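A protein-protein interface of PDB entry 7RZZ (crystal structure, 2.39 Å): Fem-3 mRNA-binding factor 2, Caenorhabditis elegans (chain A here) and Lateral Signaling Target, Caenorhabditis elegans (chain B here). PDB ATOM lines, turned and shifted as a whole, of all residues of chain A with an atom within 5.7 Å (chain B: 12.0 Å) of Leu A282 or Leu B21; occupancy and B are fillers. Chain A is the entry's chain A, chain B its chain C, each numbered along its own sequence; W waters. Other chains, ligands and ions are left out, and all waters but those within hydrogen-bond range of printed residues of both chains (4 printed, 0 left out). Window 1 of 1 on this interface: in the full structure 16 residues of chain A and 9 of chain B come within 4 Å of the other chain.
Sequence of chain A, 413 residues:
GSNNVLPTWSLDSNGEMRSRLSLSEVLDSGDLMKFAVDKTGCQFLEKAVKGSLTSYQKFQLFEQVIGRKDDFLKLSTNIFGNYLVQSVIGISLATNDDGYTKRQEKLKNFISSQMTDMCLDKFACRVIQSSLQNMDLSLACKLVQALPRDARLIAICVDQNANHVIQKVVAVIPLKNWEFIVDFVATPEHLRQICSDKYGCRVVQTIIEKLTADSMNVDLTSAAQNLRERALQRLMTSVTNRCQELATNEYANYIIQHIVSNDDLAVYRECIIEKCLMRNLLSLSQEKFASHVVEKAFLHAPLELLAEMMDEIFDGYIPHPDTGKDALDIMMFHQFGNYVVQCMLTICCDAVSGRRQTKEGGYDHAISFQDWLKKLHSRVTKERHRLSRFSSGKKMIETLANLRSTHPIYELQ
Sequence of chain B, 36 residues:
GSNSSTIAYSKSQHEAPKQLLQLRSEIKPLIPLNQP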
ATOM      1  N   ASN A 280     -21.726 -11.981  20.809  1.00  0.00           N
ATOM      2  CA  ASN A 280     -22.420 -13.179  20.347  1.00  0.00           C
ATOM      3  C   ASN A 280     -23.902 -13.147  20.697  1.00  0.00           C
ATOM      4  O   ASN A 280     -24.567 -14.185  20.634  1.00  0.00           O
ATOM      5  CB  ASN A 280     -21.786 -14.446  20.932  1.00  0.00           C
ATOM      6  CG  ASN A 280     -20.381 -14.690  20.421  1.00  0.00           C
ATOM      7  OD1 ASN A 280     -20.189 -15.200  19.318  1.00  0.00           O
ATOM      8  ND2 ASN A 280     -19.390 -14.337  21.230  1.00  0.00           N
ATOM      9  N   LEU A 281     -24.434 -11.981  21.070  1.00  0.00           N
ATOM     10  CA  LEU A 281     -25.797 -11.928  21.591  1.00  0.00           C
ATOM     11  C   LEU A 281     -26.821 -12.319  20.531  1.00  0.00           C
ATOM     12  O   LEU A 281     -27.788 -13.026  20.832  1.00  0.00           O
ATOM     13  CB  LEU A 281     -26.094 -10.534  22.139  1.00  0.00           C
ATOM     14  CG  LEU A 281     -25.213 -10.057  23.295  1.00  0.00           C
ATOM     15  CD1 LEU A 281     -25.671  -8.685  23.793  1.00  0.00           C
ATOM     16  CD2 LEU A 281     -25.223 -11.074  24.422  1.00  0.00           C
ATOM     17  N   LEU A 282     -26.631 -11.872  19.287  1.00  0.00           N
ATOM     18  CA  LEU A 282     -27.578 -12.229  18.234  1.00  0.00           C
ATOM     19  C   LEU A 282     -27.568 -13.729  17.971  1.00  0.00           C
ATOM     20  O   LEU A 282     -28.626 -14.342  17.784  1.00  0.00           O
ATOM     21  CB  LEU A 282     -27.260 -11.460  16.951  1.00  0.00           C
ATOM     22  CG  LEU A 282     -28.094 -11.837  15.723  1.00  0.00           C
ATOM     23  CD1 LEU A 282     -29.557 -11.477  15.936  1.00  0.00           C
ATOM     24  CD2 LEU A 282     -27.551 -11.164  14.468  1.00  0.00           C
ATOM     25  N   SER A 283     -26.381 -14.339  17.967  1.00  0.00           N
ATOM     26  CA  SER A 283     -26.283 -15.768  17.693  1.00  0.00           C
ATOM     27  C   SER A 283     -26.827 -16.594  18.851  1.00  0.00           C
ATOM     28  O   SER A 283     -27.557 -17.569  18.637  1.00  0.00           O
ATOM     29  CB  SER A 283     -24.832 -16.146  17.403  1.00  0.00           C
ATOM     30  OG  SER A 283     -24.699 -17.539  17.200  1.00  0.00           O
ATOM     31  N   LEU A 284     -26.482 -16.220  20.085  1.00  0.00           N
ATOM     32  CA  LEU A 284     -26.891 -17.013  21.237  1.00  0.00           C
ATOM     33  C   LEU A 284     -28.376 -16.847  21.540  1.00  0.00           C
ATOM     34  O   LEU A 284     -29.003 -17.770  22.070  1.00  0.00           O
ATOM     35  CB  LEU A 284     -26.052 -16.636  22.458  1.00  0.00           C
ATOM     36  CG  LEU A 284     -24.547 -16.899  22.345  1.00  0.00           C
ATOM     37  CD1 LEU A 284     -23.832 -16.505  23.631  1.00  0.00           C
ATOM     38  CD2 LEU A 284     -24.267 -18.352  21.988  1.00  0.00           C
ATOM     39  N   SER A 285     -28.955 -15.691  21.206  1.00  0.00           N
ATOM     40  CA  SER A 285     -30.376 -15.475  21.454  1.00  0.00           C
ATOM     41  C   SER A 285     -31.255 -16.348  20.570  1.00  0.00           C
ATOM     42  O   SER A 285     -32.442 -16.514  20.869  1.00  0.00           O
ATOM     43  CB  SER A 285     -30.732 -14.003  21.242  1.00  0.00           C
ATOM     44  OG  SER A 285     -29.952 -13.163  22.078  1.00  0.00           O
ATOM     45  N   GLN A 286     -30.706 -16.907  19.495  1.00  0.00           N
ATOM     46  CA  GLN A 286     -31.444 -17.802  18.617  1.00  0.00           C
ATOM     47  C   GLN A 286     -31.196 -19.268  18.942  1.00  0.00           C
ATOM     48  O   GLN A 286     -31.531 -20.140  18.135  1.00  0.00           O
ATOM     49  CB  GLN A 286     -31.089 -17.510  17.158  1.00  0.00           C
ATOM     50  CG  GLN A 286     -31.478 -16.102  16.718  1.00  0.00           C
ATOM     51  CD  GLN A 286     -31.009 -15.778  15.314  1.00  0.00           C
ATOM     52  OE1 GLN A 286     -31.507 -16.334  14.334  1.00  0.00           O
ATOM     53  NE2 GLN A 286     -30.046 -14.870  15.208  1.00  0.00           N
ATOM     54  N   GLU A 312     -25.170  -3.421  21.657  1.00  0.00           N
ATOM     55  CA  GLU A 312     -24.893  -4.477  20.689  1.00  0.00           C
ATOM     56  C   GLU A 312     -26.159  -4.889  19.950  1.00  0.00           C
ATOM     57  O   GLU A 312     -26.134  -5.093  18.732  1.00  0.00           O
ATOM     58  CB  GLU A 312     -24.258  -5.691  21.369  1.00  0.00           C
ATOM     59  CG  GLU A 312     -23.953  -6.821  20.382  1.00  0.00           C
ATOM     60  CD  GLU A 312     -23.237  -8.004  21.013  1.00  0.00           C
ATOM     61  OE1 GLU A 312     -22.494  -7.810  21.998  1.00  0.00           O
ATOM     62  OE2 GLU A 312     -23.417  -9.136  20.513  1.00  0.00           O
ATOM     63  N   ILE A 313     -27.278  -5.013  20.667  1.00  0.00           N
ATOM     64  CA  ILE A 313     -28.528  -5.378  20.011  1.00  0.00           C
ATOM     65  C   ILE A 313     -29.010  -4.249  19.107  1.00  0.00           C
ATOM     66  O   ILE A 313     -29.429  -4.484  17.967  1.00  0.00           O
ATOM     67  CB  ILE A 313     -29.593  -5.755  21.056  1.00  0.00           C
ATOM     68  CG1 ILE A 313     -29.089  -6.890  21.947  1.00  0.00           C
ATOM     69  CG2 ILE A 313     -30.881  -6.165  20.364  1.00  0.00           C
ATOM     70  CD1 ILE A 313     -28.587  -8.092  21.173  1.00  0.00           C
ATOM     71  N   TYR A 317     -24.593  -4.656  14.998  1.00  0.00           N
ATOM     72  CA  TYR A 317     -24.573  -5.472  13.794  1.00  0.00           C
ATOM     73  C   TYR A 317     -24.963  -4.639  12.581  1.00  0.00           C
ATOM     74  O   TYR A 317     -25.785  -3.722  12.670  1.00  0.00           O
ATOM     75  CB  TYR A 317     -25.518  -6.676  13.920  1.00  0.00           C
ATOM     76  CG  TYR A 317     -25.182  -7.603  15.066  1.00  0.00           C
ATOM     77  CD1 TYR A 317     -24.325  -8.679  14.885  1.00  0.00           C
ATOM     78  CD2 TYR A 317     -25.722  -7.403  16.330  1.00  0.00           C
ATOM     79  CE1 TYR A 317     -24.012  -9.531  15.930  1.00  0.00           C
ATOM     80  CE2 TYR A 317     -25.416  -8.250  17.383  1.00  0.00           C
ATOM     81  CZ  TYR A 317     -24.561  -9.313  17.176  1.00  0.00           C
ATOM     82  OH  TYR A 317     -24.254 -10.163  18.217  1.00  0.00           O
ATOM     83  N   ILE A 318     -24.361  -4.971  11.447  1.00  0.00           N
ATOM     84  CA  ILE A 318     -24.711  -4.330  10.178  1.00  0.00           C
ATOM     85  C   ILE A 318     -25.980  -4.983   9.636  1.00  0.00           C
ATOM     86  O   ILE A 318     -26.061  -6.221   9.602  1.00  0.00           O
ATOM     87  CB  ILE A 318     -23.561  -4.450   9.181  1.00  0.00           C
ATOM     88  CG1 ILE A 318     -22.271  -3.881   9.779  1.00  0.00           C
ATOM     89  CG2 ILE A 318     -23.900  -3.749   7.876  1.00  0.00           C
ATOM     90  CD1 ILE A 318     -22.331  -2.401  10.056  1.00  0.00           C
ATOM     91  N   PRO A 319     -26.981  -4.204   9.220  1.00  0.00           N
ATOM     92  CA  PRO A 319     -28.211  -4.805   8.689  1.00  0.00           C
ATOM     93  C   PRO A 319     -27.939  -5.644   7.449  1.00  0.00           C
ATOM     94  O   PRO A 319     -26.949  -5.452   6.738  1.00  0.00           O
ATOM     95  CB  PRO A 319     -29.090  -3.590   8.355  1.00  0.00           C
ATOM     96  CG  PRO A 319     -28.534  -2.473   9.185  1.00  0.00           C
ATOM     97  CD  PRO A 319     -27.060  -2.736   9.284  1.00  0.00           C
ATOM     98  N   HIS A 320     -28.841  -6.588   7.201  1.00  0.00           N
ATOM     99  CA  HIS A 320     -28.697  -7.491   6.068  1.00  0.00           C
ATOM    100  C   HIS A 320     -28.640  -6.689   4.769  1.00  0.00           C
ATOM    101  O   HIS A 320     -29.495  -5.822   4.545  1.00  0.00           O
ATOM    102  CB  HIS A 320     -29.858  -8.485   6.033  1.00  0.00           C
ATOM    103  CG  HIS A 320     -29.672  -9.602   5.053  1.00  0.00           C
ATOM    104  ND1 HIS A 320     -29.875  -9.446   3.698  1.00  0.00           N
ATOM    105  CD2 HIS A 320     -29.309 -10.893   5.234  1.00  0.00           C
ATOM    106  CE1 HIS A 320     -29.642 -10.594   3.087  1.00  0.00           C
ATOM    107  NE2 HIS A 320     -29.298 -11.488   3.996  1.00  0.00           N
ATOM    108  N   LYS A 325     -32.881  -5.979   7.143  1.00  0.00           N
ATOM    109  CA  LYS A 325     -33.245  -6.542   8.437  1.00  0.00           C
ATOM    110  C   LYS A 325     -32.066  -6.445   9.398  1.00  0.00           C
ATOM    111  O   LYS A 325     -30.941  -6.819   9.054  1.00  0.00           O
ATOM    112  CB  LYS A 325     -33.680  -7.998   8.265  1.00  0.00           C
ATOM    113  CG  LYS A 325     -34.313  -8.621   9.495  1.00  0.00           C
ATOM    114  CD  LYS A 325     -34.728 -10.063   9.239  1.00  0.00           C
ATOM    115  CE  LYS A 325     -35.747 -10.164   8.116  1.00  0.00           C
ATOM    116  NZ  LYS A 325     -36.180 -11.574   7.895  1.00  0.00           N
ATOM    117  N   ASP A 326     -32.321  -5.939  10.604  1.00  0.00           N
ATOM    118  CA  ASP A 326     -31.279  -5.742  11.601  1.00  0.00           C
ATOM    119  C   ASP A 326     -31.430  -6.757  12.734  1.00  0.00           C
ATOM    120  O   ASP A 326     -32.324  -7.607  12.728  1.00  0.00           O
ATOM    121  CB  ASP A 326     -31.287  -4.297  12.119  1.00  0.00           C
ATOM    122  CG  ASP A 326     -32.626  -3.871  12.704  1.00  0.00           C
ATOM    123  OD1 ASP A 326     -33.411  -4.732  13.156  1.00  0.00           O
ATOM    124  OD2 ASP A 326     -32.892  -2.651  12.717  1.00  0.00           O
ATOM    125  N   ALA A 327     -30.531  -6.655  13.718  1.00  0.00           N
ATOM    126  CA  ALA A 327     -30.486  -7.644  14.791  1.00  0.00           C
ATOM    127  C   ALA A 327     -31.759  -7.619  15.626  1.00  0.00           C
ATOM    128  O   ALA A 327     -32.249  -8.673  16.047  1.00  0.00           O
ATOM    129  CB  ALA A 327     -29.262  -7.408  15.675  1.00  0.00           C
ATOM    130  N   ILE A 330     -34.498  -9.525  13.766  1.00  0.00           N
ATOM    131  CA  ILE A 330     -34.323 -10.973  13.806  1.00  0.00           C
ATOM    132  C   ILE A 330     -34.719 -11.520  15.170  1.00  0.00           C
ATOM    133  O   ILE A 330     -35.456 -12.507  15.275  1.00  0.00           O
ATOM    134  CB  ILE A 330     -32.871 -11.347  13.449  1.00  0.00           C
ATOM    135  CG1 ILE A 330     -32.599 -11.094  11.967  1.00  0.00           C
ATOM    136  CG2 ILE A 330     -32.581 -12.799  13.797  1.00  0.00           C
ATOM    137  CD1 ILE A 330     -31.130 -11.122  11.605  1.00  0.00           C
ATOM    138  N   MET A 331     -34.243 -10.876  16.236  1.00  0.00           N
ATOM    139  CA  MET A 331     -34.503 -11.371  17.582  1.00  0.00           C
ATOM    140  C   MET A 331     -35.970 -11.202  17.956  1.00  0.00           C
ATOM    141  O   MET A 331     -36.550 -12.060  18.629  1.00  0.00           O
ATOM    142  CB  MET A 331     -33.608 -10.640  18.578  1.00  0.00           C
ATOM    143  CG  MET A 331     -32.143 -11.016  18.476  1.00  0.00           C
ATOM    144  SD  MET A 331     -31.104 -10.138  19.657  1.00  0.00           S
ATOM    145  CE  MET A 331     -32.211  -9.993  21.060  1.00  0.00           C
ATOM    146  N   GLU B  15     -35.862 -26.556  14.393  1.00  0.00           N
ATOM    147  CA  GLU B  15     -35.877 -25.104  14.484  1.00  0.00           C
ATOM    148  C   GLU B  15     -35.528 -24.472  13.142  1.00  0.00           C
ATOM    149  O   GLU B  15     -35.020 -25.124  12.226  1.00  0.00           O
ATOM    150  CB  GLU B  15     -34.903 -24.619  15.565  1.00  0.00           C
ATOM    151  CG  GLU B  15     -35.109 -25.265  16.925  1.00  0.00           C
ATOM    152  CD  GLU B  15     -33.805 -25.534  17.650  1.00  0.00           C
ATOM    153  OE1 GLU B  15     -33.741 -26.520  18.414  1.00  0.00           O
ATOM    154  OE2 GLU B  15     -32.843 -24.762  17.450  1.00  0.00           O
ATOM    155  N   ALA B  16     -35.817 -23.177  13.041  1.00  0.00           N
ATOM    156  CA  ALA B  16     -35.453 -22.398  11.871  1.00  0.00           C
ATOM    157  C   ALA B  16     -33.959 -22.086  11.892  1.00  0.00           C
ATOM    158  O   ALA B  16     -33.366 -21.924  12.963  1.00  0.00           O
ATOM    159  CB  ALA B  16     -36.251 -21.100  11.826  1.00  0.00           C
ATOM    160  N   PRO B  17     -33.326 -21.998  10.722  1.00  0.00           N
ATOM    161  CA  PRO B  17     -31.890 -21.703  10.690  1.00  0.00           C
ATOM    162  C   PRO B  17     -31.600 -20.325  11.267  1.00  0.00           C
ATOM    163  O   PRO B  17     -32.409 -19.401  11.168  1.00  0.00           O
ATOM    164  CB  PRO B  17     -31.542 -21.772   9.199  1.00  0.00           C
ATOM    165  CG  PRO B  17     -32.836 -21.522   8.495  1.00  0.00           C
ATOM    166  CD  PRO B  17     -33.897 -22.123   9.370  1.00  0.00           C
ATOM    167  N   LYS B  18     -30.430 -20.204  11.889  1.00  0.00           N
ATOM    168  CA  LYS B  18     -30.028 -18.934  12.475  1.00  0.00           C
ATOM    169  C   LYS B  18     -29.845 -17.880  11.392  1.00  0.00           C
ATOM    170  O   LYS B  18     -29.372 -18.170  10.289  1.00  0.00           O
ATOM    171  CB  LYS B  18     -28.730 -19.102  13.267  1.00  0.00           C
ATOM    172  CG  LYS B  18     -28.853 -20.004  14.482  1.00  0.00           C
ATOM    173  CD  LYS B  18     -27.488 -20.386  15.022  1.00  0.00           C
ATOM    174  CE  LYS B  18     -27.348 -20.033  16.491  1.00  0.00           C
ATOM    175  NZ  LYS B  18     -25.922 -19.831  16.870  1.00  0.00           N
ATOM    176  N   GLN B  19     -30.232 -16.653  11.710  1.00  0.00           N
ATOM    177  CA  GLN B  19     -30.038 -15.502  10.834  1.00  0.00           C
ATOM    178  C   GLN B  19     -28.907 -14.672  11.432  1.00  0.00           C
ATOM    179  O   GLN B  19     -29.106 -13.952  12.415  1.00  0.00           O
ATOM    180  CB  GLN B  19     -31.324 -14.694  10.703  1.00  0.00           C
ATOM    181  CG  GLN B  19     -32.381 -15.343   9.830  1.00  0.00           C
ATOM    182  CD  GLN B  19     -33.582 -14.446   9.616  1.00  0.00           C
ATOM    183  OE1 GLN B  19     -33.563 -13.556   8.766  1.00  0.00           O
ATOM    184  NE2 GLN B  19     -34.636 -14.673  10.394  1.00  0.00           N
ATOM    185  N   LEU B  20     -27.722 -14.778  10.843  1.00  0.00           N
ATOM    186  CA  LEU B  20     -26.538 -14.105  11.352  1.00  0.00           C
ATOM    187  C   LEU B  20     -26.312 -12.790  10.618  1.00  0.00           C
ATOM    188  O   LEU B  20     -26.655 -12.645   9.442  1.00  0.00           O
ATOM    189  CB  LEU B  20     -25.301 -14.996  11.213  1.00  0.00           C
ATOM    190  CG  LEU B  20     -24.888 -15.808  12.444  1.00  0.00           C
ATOM    191  CD1 LEU B  20     -26.089 -16.476  13.088  1.00  0.00           C
ATOM    192  CD2 LEU B  20     -23.833 -16.841  12.075  1.00  0.00           C
ATOM    193  N   LEU B  21     -25.726 -11.830  11.329  1.00  0.00           N
ATOM    194  CA  LEU B  21     -25.395 -10.530  10.768  1.00  0.00           C
ATOM    195  C   LEU B  21     -23.937 -10.210  11.051  1.00  0.00           C
ATOM    196  O   LEU B  21     -23.358 -10.687  12.031  1.00  0.00           O
ATOM    197  CB  LEU B  21     -26.285  -9.418  11.341  1.00  0.00           C
ATOM    198  CG  LEU B  21     -27.781  -9.494  11.028  1.00  0.00           C
ATOM    199  CD1 LEU B  21     -28.509  -8.314  11.653  1.00  0.00           C
ATOM    200  CD2 LEU B  21     -28.016  -9.541   9.531  1.00  0.00           C
ATOM    201  N   GLN B  22     -23.349  -9.392  10.183  1.00  0.00           N
ATOM    202  CA  GLN B  22     -21.962  -8.985  10.355  1.00  0.00           C
ATOM    203  C   GLN B  22     -21.819  -8.099  11.587  1.00  0.00           C
ATOM    204  O   GLN B  22     -22.591  -7.156  11.782  1.00  0.00           O
ATOM    205  CB  GLN B  22     -21.469  -8.254   9.109  1.00  0.00           C
ATOM    206  CG  GLN B  22     -19.959  -8.089   9.037  1.00  0.00           C
ATOM    207  CD  GLN B  22     -19.540  -6.889   8.208  1.00  0.00           C
ATOM    208  OE1 GLN B  22     -20.200  -6.536   7.229  1.00  0.00           O
ATOM    209  NE2 GLN B  22     -18.438  -6.254   8.596  1.00  0.00           N
ATOM    210  N   LEU B  23     -20.829  -8.410  12.420  1.00  0.00           N
ATOM    211  CA  LEU B  23     -20.564  -7.640  13.627  1.00  0.00           C
ATOM    212  C   LEU B  23     -19.878  -6.325  13.283  1.00  0.00           C
ATOM    213  O   LEU B  23     -19.082  -6.250  12.344  1.00  0.00           O
ATOM    214  CB  LEU B  23     -19.673  -8.436  14.581  1.00  0.00           C
ATOM    215  CG  LEU B  23     -20.239  -9.049  15.860  1.00  0.00           C
ATOM    216  CD1 LEU B  23     -19.155  -9.874  16.536  1.00  0.00           C
ATOM    217  CD2 LEU B  23     -20.774  -7.985  16.807  1.00  0.00           C
ATOM    218  N   ARG B  24     -20.183  -5.287  14.058  1.00  0.00           N
ATOM    219  CA  ARG B  24     -19.422  -4.052  13.957  1.00  0.00           C
ATOM    220  C   ARG B  24     -18.050  -4.237  14.593  1.00  0.00           C
ATOM    221  O   ARG B  24     -17.886  -4.974  15.569  1.00  0.00           O
ATOM    222  CB  ARG B  24     -20.170  -2.901  14.627  1.00  0.00           C
ATOM    223  CG  ARG B  24     -20.833  -1.958  13.637  1.00  0.00           C
ATOM    224  CD  ARG B  24     -21.297  -0.666  14.303  1.00  0.00           C
ATOM    225  NE  ARG B  24     -22.160   0.146  13.448  1.00  0.00           N
ATOM    226  CZ  ARG B  24     -21.883   0.538  12.209  1.00  0.00           C
ATOM    227  NH1 ARG B  24     -20.705   0.310  11.653  1.00  0.00           N
ATOM    228  NH2 ARG B  24     -22.807   1.202  11.520  1.00  0.00           N
ATOM    229  N   SER B  25     -17.054  -3.563  14.022  1.00  0.00           N
ATOM    230  CA  SER B  25     -15.685  -3.731  14.484  1.00  0.00           C
ATOM    231  C   SER B  25     -15.506  -3.143  15.879  1.00  0.00           C
ATOM    232  O   SER B  25     -16.142  -2.153  16.252  1.00  0.00           O
ATOM    233  CB  SER B  25     -14.706  -3.079  13.509  1.00  0.00           C
ATOM    234  OG  SER B  25     -14.264  -4.008  12.532  1.00  0.00           O
HETATM  235  O   HOH W   1     -24.759  -8.095   8.168  1.00  0.00           O
HETATM  236  O   HOH W   2     -31.668 -22.165  16.488  1.00  0.00           O
HETATM  237  O   HOH W   3     -25.057  -0.914  12.475  1.00  0.00           O
HETATM  238  O   HOH W   4     -36.330 -13.562  13.033  1.00  0.00           O
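The backbone NH (N) of Ile A318 lies within hydrogen-bond range of the backbone carbonyl oxygen (O) of Gln B22 (2.8 Å).
NZ of Lys B18 sits at hydrogen-bond distance from OG of Ser A283.
The side-chain amide oxygen (OE1) of Gln B19 sits at hydrogen-bond distance from the side-chain amino group (NZ) of Lys A325 (3.4 Å).
OE1 of Gln A286 is in hydrogen-bond range of N of Gln B19, at 2.9 Å.
Of the 18 printed residues of chain A, 10 touch a printed residue of chain B.
Hydrophobic or aromatic side chains of chain A that line the printed part of chain B: Leu A282, Tyr A317, Ile A318 and Ile A330.
Among the printed residues, 18 pairs touch across the chains.
Among the printed residues, no Asp or Glu carboxylate lies within 4 Å of a Lys or Arg side-chain nitrogen of the other chain.
Among the printed residues, pairs that only touch across the chains: Tyr A317 with Gln B22 (3.3 Å), Ala A327 with Leu B21 (3.3 Å), Asp A326 with Leu B21 (3.5 Å), Gln A286 with Lys B18 (3.5 Å), Ile A318 with Arg B24 (3.5 Å), Ile A330 with Gln B19 (3.6 Å), Tyr A317 with Leu B21 (3.6 Å), Ile A318 with Leu B21 (3.6 Å), Leu A282 with Leu B21 (3.7 Å), Tyr A317 with Leu B23 (3.7 Å), Ile A330 with Leu B21 (3.8 Å), Leu A282 with Gln B19 (3.8 Å), His A320 with Leu B21 (3.9 Å) and Lys A325 with Leu B21 (3.9 Å).
OH of Tyr A317 sits at hydrogen-bond distance from OE2 of Glu A312, 2.7 Å away.
The side-chain amide nitrogen (NE2) of Gln A286 sits at hydrogen-bond distance from the backbone carbonyl oxygen (O) of Leu A282, at 3.0 Å.
The backbone NH of Leu A281 sits at hydrogen-bond distance from the side-chain hydroxyl of Tyr A317 (3.4 Å).
The backbone NH of His A320 lies within hydrogen-bond range of the backbone carbonyl oxygen of Lys A325, 2.8 Å away.
The backbone NH (N) of Leu A282 sits at hydrogen-bond distance from the side-chain hydroxyl (OH) of Tyr A317 (3.1 Å).
Water W2 bridges the backbone carbonyl oxygen (O) of Gln A286 (2.6 Å) and the side-chain carboxylate (OE2) of Glu B15 (3.0 Å).
Water W4 bridges the backbone carbonyl oxygen (O) of Ile A330 (2.6 Å) and the side-chain amide nitrogen (NE2) of Gln B19 (3.3 Å).
Water W1 bridges O of Ile A318 (2.7 Å) and N of Gln B22 (2.8 Å).
Water W3 lies within hydrogen-bond range of the backbone carbonyl oxygen of Tyr A317 and the guanidinium group of Arg B24.
Leu A282 touches just these residues of chain B: Gln B19 and Leu B21.
Leu B21 touches just these residues of chain A: Leu A282, Tyr A317, Ile A318, His A320, Lys A325, Asp A326, Ala A327 and Ile A330.
No residue of chain B comes within 4 Å of Asn A280.
No residue of chain B comes within 4 Å of Leu A281.
Printed residues of chain B within 4 Å of Ser A283: Lys B18 (2.6 Å).
No residue of chain B comes within 4 Å of Leu A284.
No residue of chain B comes within 4 Å of Ser A285.
Ile A313 touches none of the printed residues of chain B.
Of the printed residues of chain B, Tyr A317 touches Leu B21, Gln B22 and Leu B23.
Pro A319 touches none of the printed residues of chain B.
His A320 touches just one residue of chain B: Leu B21.
Asp A326 touches just one residue of chain B: Leu B21.
Ala A327 touches one residue of chain B.
Of chain B, only Gln B19 and Leu B21 come within 4 Å of Ile A330.
No residue of chain B comes within 4 Å of Met A331.
Printed residues of chain A within 4 Å of Arg B24: Ile A318.
Of the printed residues of chain A, Gln B19 touches Leu A282 (3.8 Å), Gln A286 (2.9 Å), Lys A325 (3.4 Å) and Ile A330 (3.6 Å).
Of the printed residues of chain B, Lys A325 touches Gln B19 and Leu B21.
The nearest residue of chain B that does not touch Leu A282 is Leu B20 (4.4 Å).
The nearest residue of chain A that does not touch Leu B21 is Pro A319 (4.4 Å).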
